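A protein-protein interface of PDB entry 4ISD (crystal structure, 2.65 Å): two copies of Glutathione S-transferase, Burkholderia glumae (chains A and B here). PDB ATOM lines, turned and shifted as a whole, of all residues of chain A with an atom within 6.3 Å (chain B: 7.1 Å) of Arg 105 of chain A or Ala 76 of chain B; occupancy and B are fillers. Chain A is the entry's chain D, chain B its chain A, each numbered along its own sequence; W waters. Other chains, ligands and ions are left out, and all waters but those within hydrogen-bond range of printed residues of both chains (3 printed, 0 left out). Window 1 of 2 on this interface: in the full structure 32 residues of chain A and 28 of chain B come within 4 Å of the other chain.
Printed residues of chain B within 4 Å of Arg 105 of chain A: Ala 76 (3.9 Å), Glu 79 (3.4 Å), Glu 83 (3.1 Å) and Arg 105 (3.98 Å).
Of the printed residues of chain A, Glu 73 of chain B touches Gln 106, Ala 109 and Trp 110.
Of the printed residues of chain B, Ala 102 of chain A touches Leu 71 and Tyr 80.
Printed residues of chain B within 4 Å of Gln 106 of chain A: Leu 71, Ser 72, Glu 73 and Ala 76.
Of the printed residues of chain B, Arg 101 of chain A touches Glu 83.
Of the printed residues of chain A, Glu 83 of chain B touches Arg 98 (3.7 Å), Arg 101 (2.9 Å) and Arg 105 (3.1 Å).
Ile 77 of chain B touches none of the printed residues of chain A.
Ser 74 of chain B touches none of the printed residues of chain A.
The nearest residue of chain A that does not touch Ala 76 of chain B is Ala 102 of chain A (4.1 Å).
The nearest printed residue of chain A that does not touch Glu 83 of chain B is Ala 102 of chain A (5.8 Å).
Water W3 lies within hydrogen-bond range of OE1 of Glu 83 of chain B (2.5 Å), O of Arg 98 of chain A (3.0 Å) and NH1 of Arg 105 of chain A (3.3 Å).
Water W2 lies within hydrogen-bond range of OE2 of Glu 83 of chain B (3.0 Å), NH2 of Arg 105 of chain A (3.1 Å), NH2 of Arg 105 of chain B (3.2 Å) and OE2 of Glu 83 of chain A (3.5 Å).
Water W1 bridges OE1 of Gln 106 of chain A and OG of Ser 72 of chain B.
N of Ser 72 of chain B sits at hydrogen-bond distance from OE1 of Gln 106 of chain A.
NH2 of Arg 105 of chain A lies within salt-bridge range of OE1 of Glu 79 of chain B.
The guanidinium group (NH2) of Arg 105 of chain B is in salt-bridge range of the side-chain carboxylate (OE1) of Glu 79 of chain A, 3.8 Å away.
The side-chain carboxylate of Glu 83 of chain B is in salt-bridge range of the guanidinium group of Arg 101 of chain A (2.9 Å).
OE2 of Glu 83 of chain B is in salt-bridge range of NH1 of Arg 105 of chain A, at 3.1 Å.
The backbone carbonyl oxygen (O) of Ala 109 of chain A lies close to the side-chain carboxylate (OE1) of Glu 73 of chain B (3.5 Å).
The guanidinium group (NH1) of Arg 105 of chain B is in salt-bridge range of the side-chain carboxylate (OE1) of Glu 83 of chain A, 3.2 Å away.
Glu 83 of chain B touches Arg 98 of chain A.
Leu 71 of chain B touches Ala 102 of chain A.
Ala 102 of chain A touches Tyr 80 of chain B (CB to CD1, 3.8 Å).
CD2 of Leu 103 of chain A touches CD1 of Leu 71 of chain B, 3.98 Å away.
Arg 105 of chain A touches Ala 76 of chain B (CB to CB, 3.9 Å).
Arg 105 of chain B touches Arg 105 of chain A (NH2 to NH2, 3.98 Å).
C of Leu 71 of chain B touches OE1 of Gln 106 of chain A, 3.8 Å away.
Glu 73 of chain B touches Gln 106 of chain A.
Ala 76 of chain B touches Gln 106 of chain A.
Glu 73 of chain B touches Trp 110 of chain A.
Glu 79 of chain A touches Arg 105 of chain B, and with the chains exchanged Arg 105 of chain A touches Glu 79 of chain B.
Glu 83 of chain A touches Arg 105 of chain B, and with the chains exchanged Arg 105 of chain A touches Glu 83 of chain B.
Arg 105 of chain B touches its own counterpart, Arg 105 of chain A.
Positions printed for both chains: 79, 83, 94, 105 and 108.
Of the 17 pairs that touch across the chains among the printed residues, 5 have their exchanged pair printed and touching as well.
Of the 17 printed residues of chain A, 10 touch a printed residue of chain B.
Printed residues of chain A that touch a printed residue of chain B: Glu 79, Glu 83, Arg 98, Arg 101, Ala 102, Leu 103, Arg 105, Gln 106, Ala 109 and Trp 110.
Hydrophobic or aromatic side chains of chain A within 4 Å of the printed part of chain B: Ala 102, Leu 103, Ala 109 and Trp 110.
Along chain A the printed residues that touch a printed residue of chain B span positions 79 to 110.
Hydrophobic or aromatic side chains of chain B that line the printed part of chain A: Leu 71, Ala 76 and Tyr 80.
N of Leu 64 of chain B sits at hydrogen-bond distance from O of Leu 71 of chain B (2.6 Å).
NE of Arg 105 of chain A is in salt-bridge range of OE2 of Glu 79 of chain A, at 2.6 Å.
The guanidinium group (NE) of Arg 105 of chain B lies within salt-bridge range of the side-chain carboxylate (OE2) of Glu 79 of chain B (3.1 Å).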
ATOM      1  N   GLU A  79      22.184  -9.922 -26.917  1.00  0.00           N
ATOM      2  CA  GLU A  79      23.536  -9.359 -27.004  1.00  0.00           C
ATOM      3  C   GLU A  79      23.734  -8.400 -28.187  1.00  0.00           C
ATOM      4  O   GLU A  79      24.364  -7.348 -28.054  1.00  0.00           O
ATOM      5  CB  GLU A  79      24.564 -10.485 -27.075  1.00  0.00           C
ATOM      6  CG  GLU A  79      24.723 -11.248 -25.775  1.00  0.00           C
ATOM      7  CD  GLU A  79      25.613 -10.518 -24.792  1.00  0.00           C
ATOM      8  OE1 GLU A  79      26.011  -9.367 -25.086  1.00  0.00           O
ATOM      9  OE2 GLU A  79      25.926 -11.101 -23.734  1.00  0.00           O
ATOM     10  N   GLU A  83      23.980  -3.992 -28.464  1.00  0.00           N
ATOM     11  CA  GLU A  83      25.106  -3.297 -29.100  1.00  0.00           C
ATOM     12  C   GLU A  83      24.635  -2.303 -30.164  1.00  0.00           C
ATOM     13  O   GLU A  83      25.079  -1.157 -30.185  1.00  0.00           O
ATOM     14  CB  GLU A  83      26.093  -4.301 -29.721  1.00  0.00           C
ATOM     15  CG  GLU A  83      27.443  -4.407 -29.000  1.00  0.00           C
ATOM     16  CD  GLU A  83      28.007  -5.820 -29.018  1.00  0.00           C
ATOM     17  OE1 GLU A  83      27.840  -6.500 -30.049  1.00  0.00           O
ATOM     18  OE2 GLU A  83      28.596  -6.259 -27.996  1.00  0.00           O
ATOM     19  N   LEU A  94      20.700  -5.634 -20.811  1.00  0.00           N
ATOM     20  CA  LEU A  94      21.794  -6.240 -20.050  1.00  0.00           C
ATOM     21  C   LEU A  94      22.340  -5.195 -19.078  1.00  0.00           C
ATOM     22  O   LEU A  94      22.233  -3.983 -19.335  1.00  0.00           O
ATOM     23  CB  LEU A  94      22.895  -6.754 -20.982  1.00  0.00           C
ATOM     24  CG  LEU A  94      22.640  -8.064 -21.741  1.00  0.00           C
ATOM     25  CD1 LEU A  94      23.800  -8.365 -22.674  1.00  0.00           C
ATOM     26  CD2 LEU A  94      22.456  -9.235 -20.798  1.00  0.00           C
ATOM     27  N   ARG A  98      30.161  -4.199 -15.411  1.00  0.00           N
ATOM     28  CA  ARG A  98      30.870  -5.254 -16.102  1.00  0.00           C
ATOM     29  C   ARG A  98      30.673  -6.641 -15.500  1.00  0.00           C
ATOM     30  O   ARG A  98      30.367  -7.590 -16.230  1.00  0.00           O
ATOM     31  CB  ARG A  98      32.345  -4.908 -16.170  1.00  0.00           C
ATOM     32  CG  ARG A  98      33.174  -5.951 -16.828  1.00  0.00           C
ATOM     33  CD  ARG A  98      34.575  -5.782 -16.368  1.00  0.00           C
ATOM     34  NE  ARG A  98      35.048  -4.441 -16.650  1.00  0.00           N
ATOM     35  CZ  ARG A  98      36.248  -4.003 -16.298  1.00  0.00           C
ATOM     36  NH1 ARG A  98      37.075  -4.806 -15.643  1.00  0.00           N
ATOM     37  NH2 ARG A  98      36.610  -2.766 -16.586  1.00  0.00           N
ATOM     38  N   THR A 100      28.314  -7.504 -13.354  1.00  0.00           N
ATOM     39  CA  THR A 100      26.904  -7.841 -13.293  1.00  0.00           C
ATOM     40  C   THR A 100      26.462  -8.351 -14.666  1.00  0.00           C
ATOM     41  O   THR A 100      25.672  -9.292 -14.759  1.00  0.00           O
ATOM     42  CB  THR A 100      26.048  -6.670 -12.745  1.00  0.00           C
ATOM     43  OG1 THR A 100      26.493  -6.339 -11.425  1.00  0.00           O
ATOM     44  CG2 THR A 100      24.612  -7.051 -12.661  1.00  0.00           C
ATOM     45  N   ARG A 101      26.977  -7.727 -15.723  1.00  0.00           N
ATOM     46  CA  ARG A 101      26.833  -8.230 -17.094  1.00  0.00           C
ATOM     47  C   ARG A 101      27.320  -9.685 -17.210  1.00  0.00           C
ATOM     48  O   ARG A 101      26.696 -10.510 -17.885  1.00  0.00           O
ATOM     49  CB  ARG A 101      27.633  -7.343 -18.054  1.00  0.00           C
ATOM     50  CG  ARG A 101      27.511  -7.674 -19.556  1.00  0.00           C
ATOM     51  CD  ARG A 101      28.297  -6.635 -20.364  1.00  0.00           C
ATOM     52  NE  ARG A 101      28.001  -5.283 -19.900  1.00  0.00           N
ATOM     53  CZ  ARG A 101      28.908  -4.361 -19.591  1.00  0.00           C
ATOM     54  NH1 ARG A 101      30.210  -4.615 -19.694  1.00  0.00           N
ATOM     55  NH2 ARG A 101      28.501  -3.168 -19.183  1.00  0.00           N
ATOM     56  N   ALA A 102      28.427 -10.006 -16.544  1.00  0.00           N
ATOM     57  CA  ALA A 102      28.925 -11.381 -16.540  1.00  0.00           C
ATOM     58  C   ALA A 102      27.891 -12.315 -15.950  1.00  0.00           C
ATOM     59  O   ALA A 102      27.546 -13.335 -16.551  1.00  0.00           O
ATOM     60  CB  ALA A 102      30.249 -11.477 -15.775  1.00  0.00           C
ATOM     61  N   LEU A 103      27.368 -11.944 -14.782  1.00  0.00           N
ATOM     62  CA  LEU A 103      26.391 -12.766 -14.058  1.00  0.00           C
ATOM     63  C   LEU A 103      25.070 -12.978 -14.802  1.00  0.00           C
ATOM     64  O   LEU A 103      24.488 -14.073 -14.752  1.00  0.00           O
ATOM     65  CB  LEU A 103      26.137 -12.187 -12.669  1.00  0.00           C
ATOM     66  CG  LEU A 103      27.362 -12.272 -11.758  1.00  0.00           C
ATOM     67  CD1 LEU A 103      27.113 -11.538 -10.471  1.00  0.00           C
ATOM     68  CD2 LEU A 103      27.737 -13.735 -11.501  1.00  0.00           C
ATOM     69  N   ALA A 104      24.581 -11.946 -15.483  1.00  0.00           N
ATOM     70  CA  ALA A 104      23.389 -12.115 -16.316  1.00  0.00           C
ATOM     71  C   ALA A 104      23.686 -13.070 -17.482  1.00  0.00           C
ATOM     72  O   ALA A 104      22.807 -13.833 -17.905  1.00  0.00           O
ATOM     73  CB  ALA A 104      22.870 -10.768 -16.825  1.00  0.00           C
ATOM     74  N   ARG A 105      24.920 -13.039 -17.992  1.00  0.00           N
ATOM     75  CA  ARG A 105      25.303 -13.957 -19.064  1.00  0.00           C
ATOM     76  C   ARG A 105      25.363 -15.388 -18.553  1.00  0.00           C
ATOM     77  O   ARG A 105      24.895 -16.324 -19.217  1.00  0.00           O
ATOM     78  CB  ARG A 105      26.638 -13.551 -19.700  1.00  0.00           C
ATOM     79  CG  ARG A 105      26.500 -12.413 -20.694  1.00  0.00           C
ATOM     80  CD  ARG A 105      27.832 -11.792 -20.976  1.00  0.00           C
ATOM     81  NE  ARG A 105      27.746 -10.728 -21.975  1.00  0.00           N
ATOM     82  CZ  ARG A 105      28.698  -9.824 -22.174  1.00  0.00           C
ATOM     83  NH1 ARG A 105      29.802  -9.846 -21.423  1.00  0.00           N
ATOM     84  NH2 ARG A 105      28.531  -8.887 -23.104  1.00  0.00           N
ATOM     85  N   GLN A 106      25.942 -15.562 -17.370  1.00  0.00           N
ATOM     86  CA  GLN A 106      25.963 -16.883 -16.755  1.00  0.00           C
ATOM     87  C   GLN A 106      24.535 -17.414 -16.604  1.00  0.00           C
ATOM     88  O   GLN A 106      24.231 -18.553 -16.992  1.00  0.00           O
ATOM     89  CB  GLN A 106      26.665 -16.830 -15.401  1.00  0.00           C
ATOM     90  CG  GLN A 106      26.234 -17.919 -14.447  1.00  0.00           C
ATOM     91  CD  GLN A 106      27.020 -17.878 -13.153  1.00  0.00           C
ATOM     92  OE1 GLN A 106      28.058 -18.528 -13.026  1.00  0.00           O
ATOM     93  NE2 GLN A 106      26.531 -17.106 -12.184  1.00  0.00           N
ATOM     94  N   LEU A 107      23.655 -16.568 -16.080  1.00  0.00           N
ATOM     95  CA  LEU A 107      22.270 -16.968 -15.817  1.00  0.00           C
ATOM     96  C   LEU A 107      21.539 -17.365 -17.096  1.00  0.00           C
ATOM     97  O   LEU A 107      20.866 -18.399 -17.127  1.00  0.00           O
ATOM     98  CB  LEU A 107      21.517 -15.847 -15.099  1.00  0.00           C
ATOM     99  CG  LEU A 107      20.116 -16.130 -14.594  1.00  0.00           C
ATOM    100  CD1 LEU A 107      20.098 -17.407 -13.801  1.00  0.00           C
ATOM    101  CD2 LEU A 107      19.663 -14.974 -13.714  1.00  0.00           C
ATOM    102  N   GLN A 108      21.667 -16.543 -18.141  1.00  0.00           N
ATOM    103  CA  GLN A 108      21.137 -16.868 -19.472  1.00  0.00           C
ATOM    104  C   GLN A 108      21.670 -18.204 -20.014  1.00  0.00           C
ATOM    105  O   GLN A 108      20.901 -19.071 -20.429  1.00  0.00           O
ATOM    106  CB  GLN A 108      21.449 -15.739 -20.471  1.00  0.00           C
ATOM    107  CG  GLN A 108      20.530 -14.531 -20.325  1.00  0.00           C
ATOM    108  CD  GLN A 108      20.400 -13.717 -21.596  1.00  0.00           C
ATOM    109  OE1 GLN A 108      21.344 -13.071 -22.023  1.00  0.00           O
ATOM    110  NE2 GLN A 108      19.218 -13.742 -22.205  1.00  0.00           N
ATOM    111  N   ALA A 109      22.984 -18.373 -20.005  1.00  0.00           N
ATOM    112  CA  ALA A 109      23.566 -19.593 -20.540  1.00  0.00           C
ATOM    113  C   ALA A 109      23.254 -20.816 -19.669  1.00  0.00           C
ATOM    114  O   ALA A 109      23.107 -21.945 -20.182  1.00  0.00           O
ATOM    115  CB  ALA A 109      25.071 -19.433 -20.751  1.00  0.00           C
ATOM    116  N   TRP A 110      23.149 -20.608 -18.357  1.00  0.00           N
ATOM    117  CA  TRP A 110      22.822 -21.729 -17.473  1.00  0.00           C
ATOM    118  C   TRP A 110      21.439 -22.241 -17.824  1.00  0.00           C
ATOM    119  O   TRP A 110      21.244 -23.438 -18.072  1.00  0.00           O
ATOM    120  CB  TRP A 110      22.869 -21.309 -16.017  1.00  0.00           C
ATOM    121  CG  TRP A 110      22.726 -22.442 -15.046  1.00  0.00           C
ATOM    122  CD1 TRP A 110      23.035 -23.754 -15.256  1.00  0.00           C
ATOM    123  CD2 TRP A 110      22.238 -22.353 -13.702  1.00  0.00           C
ATOM    124  NE1 TRP A 110      22.767 -24.489 -14.126  1.00  0.00           N
ATOM    125  CE2 TRP A 110      22.281 -23.649 -13.155  1.00  0.00           C
ATOM    126  CE3 TRP A 110      21.784 -21.300 -12.905  1.00  0.00           C
ATOM    127  CZ2 TRP A 110      21.877 -23.922 -11.849  1.00  0.00           C
ATOM    128  CZ3 TRP A 110      21.376 -21.570 -11.610  1.00  0.00           C
ATOM    129  CH2 TRP A 110      21.421 -22.871 -11.096  1.00  0.00           C
ATOM    130  N   PHE A 163      19.444  -8.634 -10.061  1.00  0.00           N
ATOM    131  CA  PHE A 163      20.640  -7.773 -10.028  1.00  0.00           C
ATOM    132  C   PHE A 163      20.277  -6.307  -9.864  1.00  0.00           C
ATOM    133  O   PHE A 163      21.037  -5.431 -10.291  1.00  0.00           O
ATOM    134  CB  PHE A 163      21.526  -7.895 -11.293  1.00  0.00           C
ATOM    135  CG  PHE A 163      21.885  -9.304 -11.669  1.00  0.00           C
ATOM    136  CD1 PHE A 163      22.732 -10.060 -10.865  1.00  0.00           C
ATOM    137  CD2 PHE A 163      21.379  -9.875 -12.837  1.00  0.00           C
ATOM    138  CE1 PHE A 163      23.075 -11.375 -11.208  1.00  0.00           C
ATOM    139  CE2 PHE A 163      21.709 -11.196 -13.195  1.00  0.00           C
ATOM    140  CZ  PHE A 163      22.561 -11.943 -12.374  1.00  0.00           C
ATOM    141  N   ALA A 169      17.767 -11.364 -18.358  1.00  0.00           N
ATOM    142  CA  ALA A 169      17.934 -12.604 -17.598  1.00  0.00           C
ATOM    143  C   ALA A 169      16.813 -12.824 -16.581  1.00  0.00           C
ATOM    144  O   ALA A 169      16.493 -13.967 -16.247  1.00  0.00           O
ATOM    145  CB  ALA A 169      19.270 -12.621 -16.891  1.00  0.00           C
ATOM    146  N   LEU B  64      35.314 -19.741 -13.104  1.00  0.00           N
ATOM    147  CA  LEU B  64      36.463 -18.840 -13.033  1.00  0.00           C
ATOM    148  C   LEU B  64      36.430 -18.020 -11.743  1.00  0.00           C
ATOM    149  O   LEU B  64      35.396 -17.478 -11.374  1.00  0.00           O
ATOM    150  CB  LEU B  64      36.488 -17.908 -14.251  1.00  0.00           C
ATOM    151  CG  LEU B  64      37.551 -16.805 -14.301  1.00  0.00           C
ATOM    152  CD1 LEU B  64      38.894 -17.334 -14.808  1.00  0.00           C
ATOM    153  CD2 LEU B  64      37.074 -15.624 -15.146  1.00  0.00           C
ATOM    154  N   LEU B  71      32.686 -16.910 -11.378  1.00  0.00           N
ATOM    155  CA  LEU B  71      31.860 -16.920 -12.577  1.00  0.00           C
ATOM    156  C   LEU B  71      31.878 -18.300 -13.228  1.00  0.00           C
ATOM    157  O   LEU B  71      32.950 -18.824 -13.533  1.00  0.00           O
ATOM    158  CB  LEU B  71      32.383 -15.873 -13.570  1.00  0.00           C
ATOM    159  CG  LEU B  71      31.500 -15.624 -14.793  1.00  0.00           C
ATOM    160  CD1 LEU B  71      30.203 -14.967 -14.373  1.00  0.00           C
ATOM    161  CD2 LEU B  71      32.199 -14.780 -15.836  1.00  0.00           C
ATOM    162  N   SER B  72      30.697 -18.886 -13.441  1.00  0.00           N
ATOM    163  CA  SER B  72      30.578 -20.152 -14.189  1.00  0.00           C
ATOM    164  C   SER B  72      30.087 -19.935 -15.632  1.00  0.00           C
ATOM    165  O   SER B  72      29.936 -18.792 -16.066  1.00  0.00           O
ATOM    166  CB  SER B  72      29.677 -21.144 -13.451  1.00  0.00           C
ATOM    167  OG  SER B  72      30.404 -21.840 -12.441  1.00  0.00           O
ATOM    168  N   GLU B  73      29.851 -21.025 -16.366  1.00  0.00           N
ATOM    169  CA  GLU B  73      29.461 -20.965 -17.785  1.00  0.00           C
ATOM    170  C   GLU B  73      30.584 -20.393 -18.660  1.00  0.00           C
ATOM    171  O   GLU B  73      30.837 -19.170 -18.663  1.00  0.00           O
ATOM    172  CB  GLU B  73      28.156 -20.191 -18.016  1.00  0.00           C
ATOM    173  CG  GLU B  73      26.926 -20.813 -17.367  1.00  0.00           C
ATOM    174  CD  GLU B  73      26.549 -22.134 -18.009  1.00  0.00           C
ATOM    175  OE1 GLU B  73      26.423 -22.147 -19.249  1.00  0.00           O
ATOM    176  OE2 GLU B  73      26.400 -23.152 -17.279  1.00  0.00           O
ATOM    177  N   SER B  74      31.224 -21.299 -19.411  1.00  0.00           N
ATOM    178  CA  SER B  74      32.426 -21.009 -20.183  1.00  0.00           C
ATOM    179  C   SER B  74      32.271 -19.869 -21.191  1.00  0.00           C
ATOM    180  O   SER B  74      33.204 -19.071 -21.377  1.00  0.00           O
ATOM    181  CB  SER B  74      32.925 -22.275 -20.885  1.00  0.00           C
ATOM    182  OG  SER B  74      32.074 -22.654 -21.949  1.00  0.00           O
ATOM    183  N   SER B  75      31.107 -19.780 -21.837  1.00  0.00           N
ATOM    184  CA  SER B  75      30.874 -18.664 -22.751  1.00  0.00           C
ATOM    185  C   SER B  75      30.858 -17.326 -21.986  1.00  0.00           C
ATOM    186  O   SER B  75      31.463 -16.349 -22.431  1.00  0.00           O
ATOM    187  CB  SER B  75      29.595 -18.859 -23.591  1.00  0.00           C
ATOM    188  OG  SER B  75      28.398 -18.672 -22.842  1.00  0.00           O
ATOM    189  N   ALA B  76      30.186 -17.288 -20.836  1.00  0.00           N
ATOM    190  CA  ALA B  76      30.151 -16.086 -20.005  1.00  0.00           C
ATOM    191  C   ALA B  76      31.555 -15.703 -19.528  1.00  0.00           C
ATOM    192  O   ALA B  76      31.901 -14.509 -19.412  1.00  0.00           O
ATOM    193  CB  ALA B  76      29.220 -16.289 -18.813  1.00  0.00           C
ATOM    194  N   ILE B  77      32.357 -16.727 -19.244  1.00  0.00           N
ATOM    195  CA  ILE B  77      33.762 -16.527 -18.936  1.00  0.00           C
ATOM    196  C   ILE B  77      34.511 -15.867 -20.105  1.00  0.00           C
ATOM    197  O   ILE B  77      35.250 -14.894 -19.902  1.00  0.00           O
ATOM    198  CB  ILE B  77      34.446 -17.854 -18.548  1.00  0.00           C
ATOM    199  CG1 ILE B  77      33.830 -18.397 -17.253  1.00  0.00           C
ATOM    200  CG2 ILE B  77      35.962 -17.658 -18.412  1.00  0.00           C
ATOM    201  CD1 ILE B  77      34.358 -19.763 -16.823  1.00  0.00           C
ATOM    202  N   ALA B  78      34.321 -16.389 -21.319  1.00  0.00           N
ATOM    203  CA  ALA B  78      34.969 -15.811 -22.499  1.00  0.00           C
ATOM    204  C   ALA B  78      34.597 -14.339 -22.702  1.00  0.00           C
ATOM    205  O   ALA B  78      35.467 -13.511 -22.999  1.00  0.00           O
ATOM    206  CB  ALA B  78      34.639 -16.614 -23.742  1.00  0.00           C
ATOM    207  N   GLU B  79      33.315 -14.020 -22.526  1.00  0.00           N
ATOM    208  CA  GLU B  79      32.803 -12.659 -22.709  1.00  0.00           C
ATOM    209  C   GLU B  79      33.399 -11.716 -21.681  1.00  0.00           C
ATOM    210  O   GLU B  79      33.670 -10.539 -21.957  1.00  0.00           O
ATOM    211  CB  GLU B  79      31.282 -12.653 -22.538  1.00  0.00           C
ATOM    212  CG  GLU B  79      30.535 -13.500 -23.542  1.00  0.00           C
ATOM    213  CD  GLU B  79      30.267 -12.757 -24.827  1.00  0.00           C
ATOM    214  OE1 GLU B  79      30.560 -11.535 -24.894  1.00  0.00           O
ATOM    215  OE2 GLU B  79      29.766 -13.397 -25.771  1.00  0.00           O
ATOM    216  N   TYR B  80      33.586 -12.249 -20.481  1.00  0.00           N
ATOM    217  CA  TYR B  80      34.045 -11.459 -19.351  1.00  0.00           C
ATOM    218  C   TYR B  80      35.546 -11.203 -19.409  1.00  0.00           C
ATOM    219  O   TYR B  80      36.003 -10.083 -19.139  1.00  0.00           O
ATOM    220  CB  TYR B  80      33.669 -12.165 -18.046  1.00  0.00           C
ATOM    221  CG  TYR B  80      34.319 -11.580 -16.821  1.00  0.00           C
ATOM    222  CD1 TYR B  80      33.843 -10.401 -16.255  1.00  0.00           C
ATOM    223  CD2 TYR B  80      35.413 -12.211 -16.222  1.00  0.00           C
ATOM    224  CE1 TYR B  80      34.440  -9.862 -15.125  1.00  0.00           C
ATOM    225  CE2 TYR B  80      36.005 -11.685 -15.092  1.00  0.00           C
ATOM    226  CZ  TYR B  80      35.521 -10.510 -14.554  1.00  0.00           C
ATOM    227  OH  TYR B  80      36.118  -9.979 -13.438  1.00  0.00           O
ATOM    228  N   LEU B  81      36.319 -12.237 -19.744  1.00  0.00           N
ATOM    229  CA  LEU B  81      37.763 -12.055 -19.893  1.00  0.00           C
ATOM    230  C   LEU B  81      38.060 -11.108 -21.059  1.00  0.00           C
ATOM    231  O   LEU B  81      38.992 -10.318 -21.000  1.00  0.00           O
ATOM    232  CB  LEU B  81      38.490 -13.389 -20.049  1.00  0.00           C
ATOM    233  CG  LEU B  81      38.506 -14.301 -18.815  1.00  0.00           C
ATOM    234  CD1 LEU B  81      39.096 -15.671 -19.168  1.00  0.00           C
ATOM    235  CD2 LEU B  81      39.284 -13.664 -17.677  1.00  0.00           C
ATOM    236  N   ASP B  82      37.224 -11.162 -22.091  1.00  0.00           N
ATOM    237  CA  ASP B  82      37.345 -10.252 -23.223  1.00  0.00           C
ATOM    238  C   ASP B  82      37.056  -8.796 -22.866  1.00  0.00           C
ATOM    239  O   ASP B  82      37.504  -7.889 -23.562  1.00  0.00           O
ATOM    240  CB  ASP B  82      36.428 -10.695 -24.361  1.00  0.00           C
ATOM    241  CG  ASP B  82      37.153 -10.781 -25.690  1.00  0.00           C
ATOM    242  OD1 ASP B  82      38.307 -11.264 -25.708  1.00  0.00           O
ATOM    243  OD2 ASP B  82      36.569 -10.362 -26.713  1.00  0.00           O
ATOM    244  N   GLU B  83      36.304  -8.566 -21.793  1.00  0.00           N
ATOM    245  CA  GLU B  83      35.967  -7.205 -21.385  1.00  0.00           C
ATOM    246  C   GLU B  83      37.001  -6.646 -20.418  1.00  0.00           C
ATOM    247  O   GLU B  83      37.336  -5.455 -20.460  1.00  0.00           O
ATOM    248  CB  GLU B  83      34.561  -7.150 -20.774  1.00  0.00           C
ATOM    249  CG  GLU B  83      33.501  -6.694 -21.762  1.00  0.00           C
ATOM    250  CD  GLU B  83      32.096  -6.993 -21.313  1.00  0.00           C
ATOM    251  OE1 GLU B  83      31.855  -7.024 -20.090  1.00  0.00           O
ATOM    252  OE2 GLU B  83      31.231  -7.213 -22.190  1.00  0.00           O
ATOM    253  N   LEU B  94      36.989 -12.916 -29.107  1.00  0.00           N
ATOM    254  CA  LEU B  94      35.759 -12.661 -29.860  1.00  0.00           C
ATOM    255  C   LEU B  94      36.009 -11.704 -31.024  1.00  0.00           C
ATOM    256  O   LEU B  94      36.787 -10.757 -30.895  1.00  0.00           O
ATOM    257  CB  LEU B  94      34.680 -12.074 -28.946  1.00  0.00           C
ATOM    258  CG  LEU B  94      33.860 -12.967 -28.010  1.00  0.00           C
ATOM    259  CD1 LEU B  94      32.688 -12.162 -27.420  1.00  0.00           C
ATOM    260  CD2 LEU B  94      33.366 -14.254 -28.716  1.00  0.00           C
ATOM    261  N   ARG B 105      28.843 -15.603 -31.036  1.00  0.00           N
ATOM    262  CA  ARG B 105      27.961 -15.769 -29.896  1.00  0.00           C
ATOM    263  C   ARG B 105      26.853 -16.775 -30.191  1.00  0.00           C
ATOM    264  O   ARG B 105      26.555 -17.660 -29.368  1.00  0.00           O
ATOM    265  CB  ARG B 105      27.372 -14.430 -29.486  1.00  0.00           C
ATOM    266  CG  ARG B 105      28.338 -13.567 -28.678  1.00  0.00           C
ATOM    267  CD  ARG B 105      27.759 -12.180 -28.510  1.00  0.00           C
ATOM    268  NE  ARG B 105      28.564 -11.315 -27.666  1.00  0.00           N
ATOM    269  CZ  ARG B 105      28.599  -9.994 -27.798  1.00  0.00           C
ATOM    270  NH1 ARG B 105      27.887  -9.405 -28.760  1.00  0.00           N
ATOM    271  NH2 ARG B 105      29.355  -9.267 -26.983  1.00  0.00           N
ATOM    272  N   GLN B 108      28.557 -20.424 -30.263  1.00  0.00           N
ATOM    273  CA  GLN B 108      28.779 -20.844 -28.867  1.00  0.00           C
ATOM    274  C   GLN B 108      27.511 -21.332 -28.164  1.00  0.00           C
ATOM    275  O   GLN B 108      27.510 -22.378 -27.521  1.00  0.00           O
ATOM    276  CB  GLN B 108      29.403 -19.707 -28.047  1.00  0.00           C
ATOM    277  CG  GLN B 108      30.834 -19.373 -28.454  1.00  0.00           C
ATOM    278  CD  GLN B 108      31.643 -18.837 -27.298  1.00  0.00           C
ATOM    279  OE1 GLN B 108      31.496 -17.670 -26.915  1.00  0.00           O
ATOM    280  NE2 GLN B 108      32.498 -19.693 -26.715  1.00  0.00           N
ATOM    281  N   ARG B 112      26.333 -25.232 -27.124  1.00  0.00           N
ATOM    282  CA  ARG B 112      26.060 -25.521 -25.735  1.00  0.00           C
ATOM    283  C   ARG B 112      24.611 -25.926 -25.438  1.00  0.00           C
ATOM    284  O   ARG B 112      24.323 -26.366 -24.318  1.00  0.00           O
ATOM    285  CB  ARG B 112      26.421 -24.295 -24.903  1.00  0.00           C
ATOM    286  CG  ARG B 112      27.910 -24.060 -24.750  1.00  0.00           C
ATOM    287  CD  ARG B 112      28.225 -22.669 -24.239  1.00  0.00           C
ATOM    288  NE  ARG B 112      29.654 -22.514 -24.000  1.00  0.00           N
ATOM    289  CZ  ARG B 112      30.576 -22.407 -24.961  1.00  0.00           C
ATOM    290  NH1 ARG B 112      30.221 -22.436 -26.252  1.00  0.00           N
ATOM    291  NH2 ARG B 112      31.861 -22.276 -24.629  1.00  0.00           N
HETATM  292  O   HOH W   1      29.023 -19.909 -10.475  1.00  0.00           O
HETATM  293  O   HOH W   2      30.040  -6.870 -24.907  1.00  0.00           O
HETATM  294  O   HOH W   3      31.387  -9.031 -18.684  1.00  0.00           O
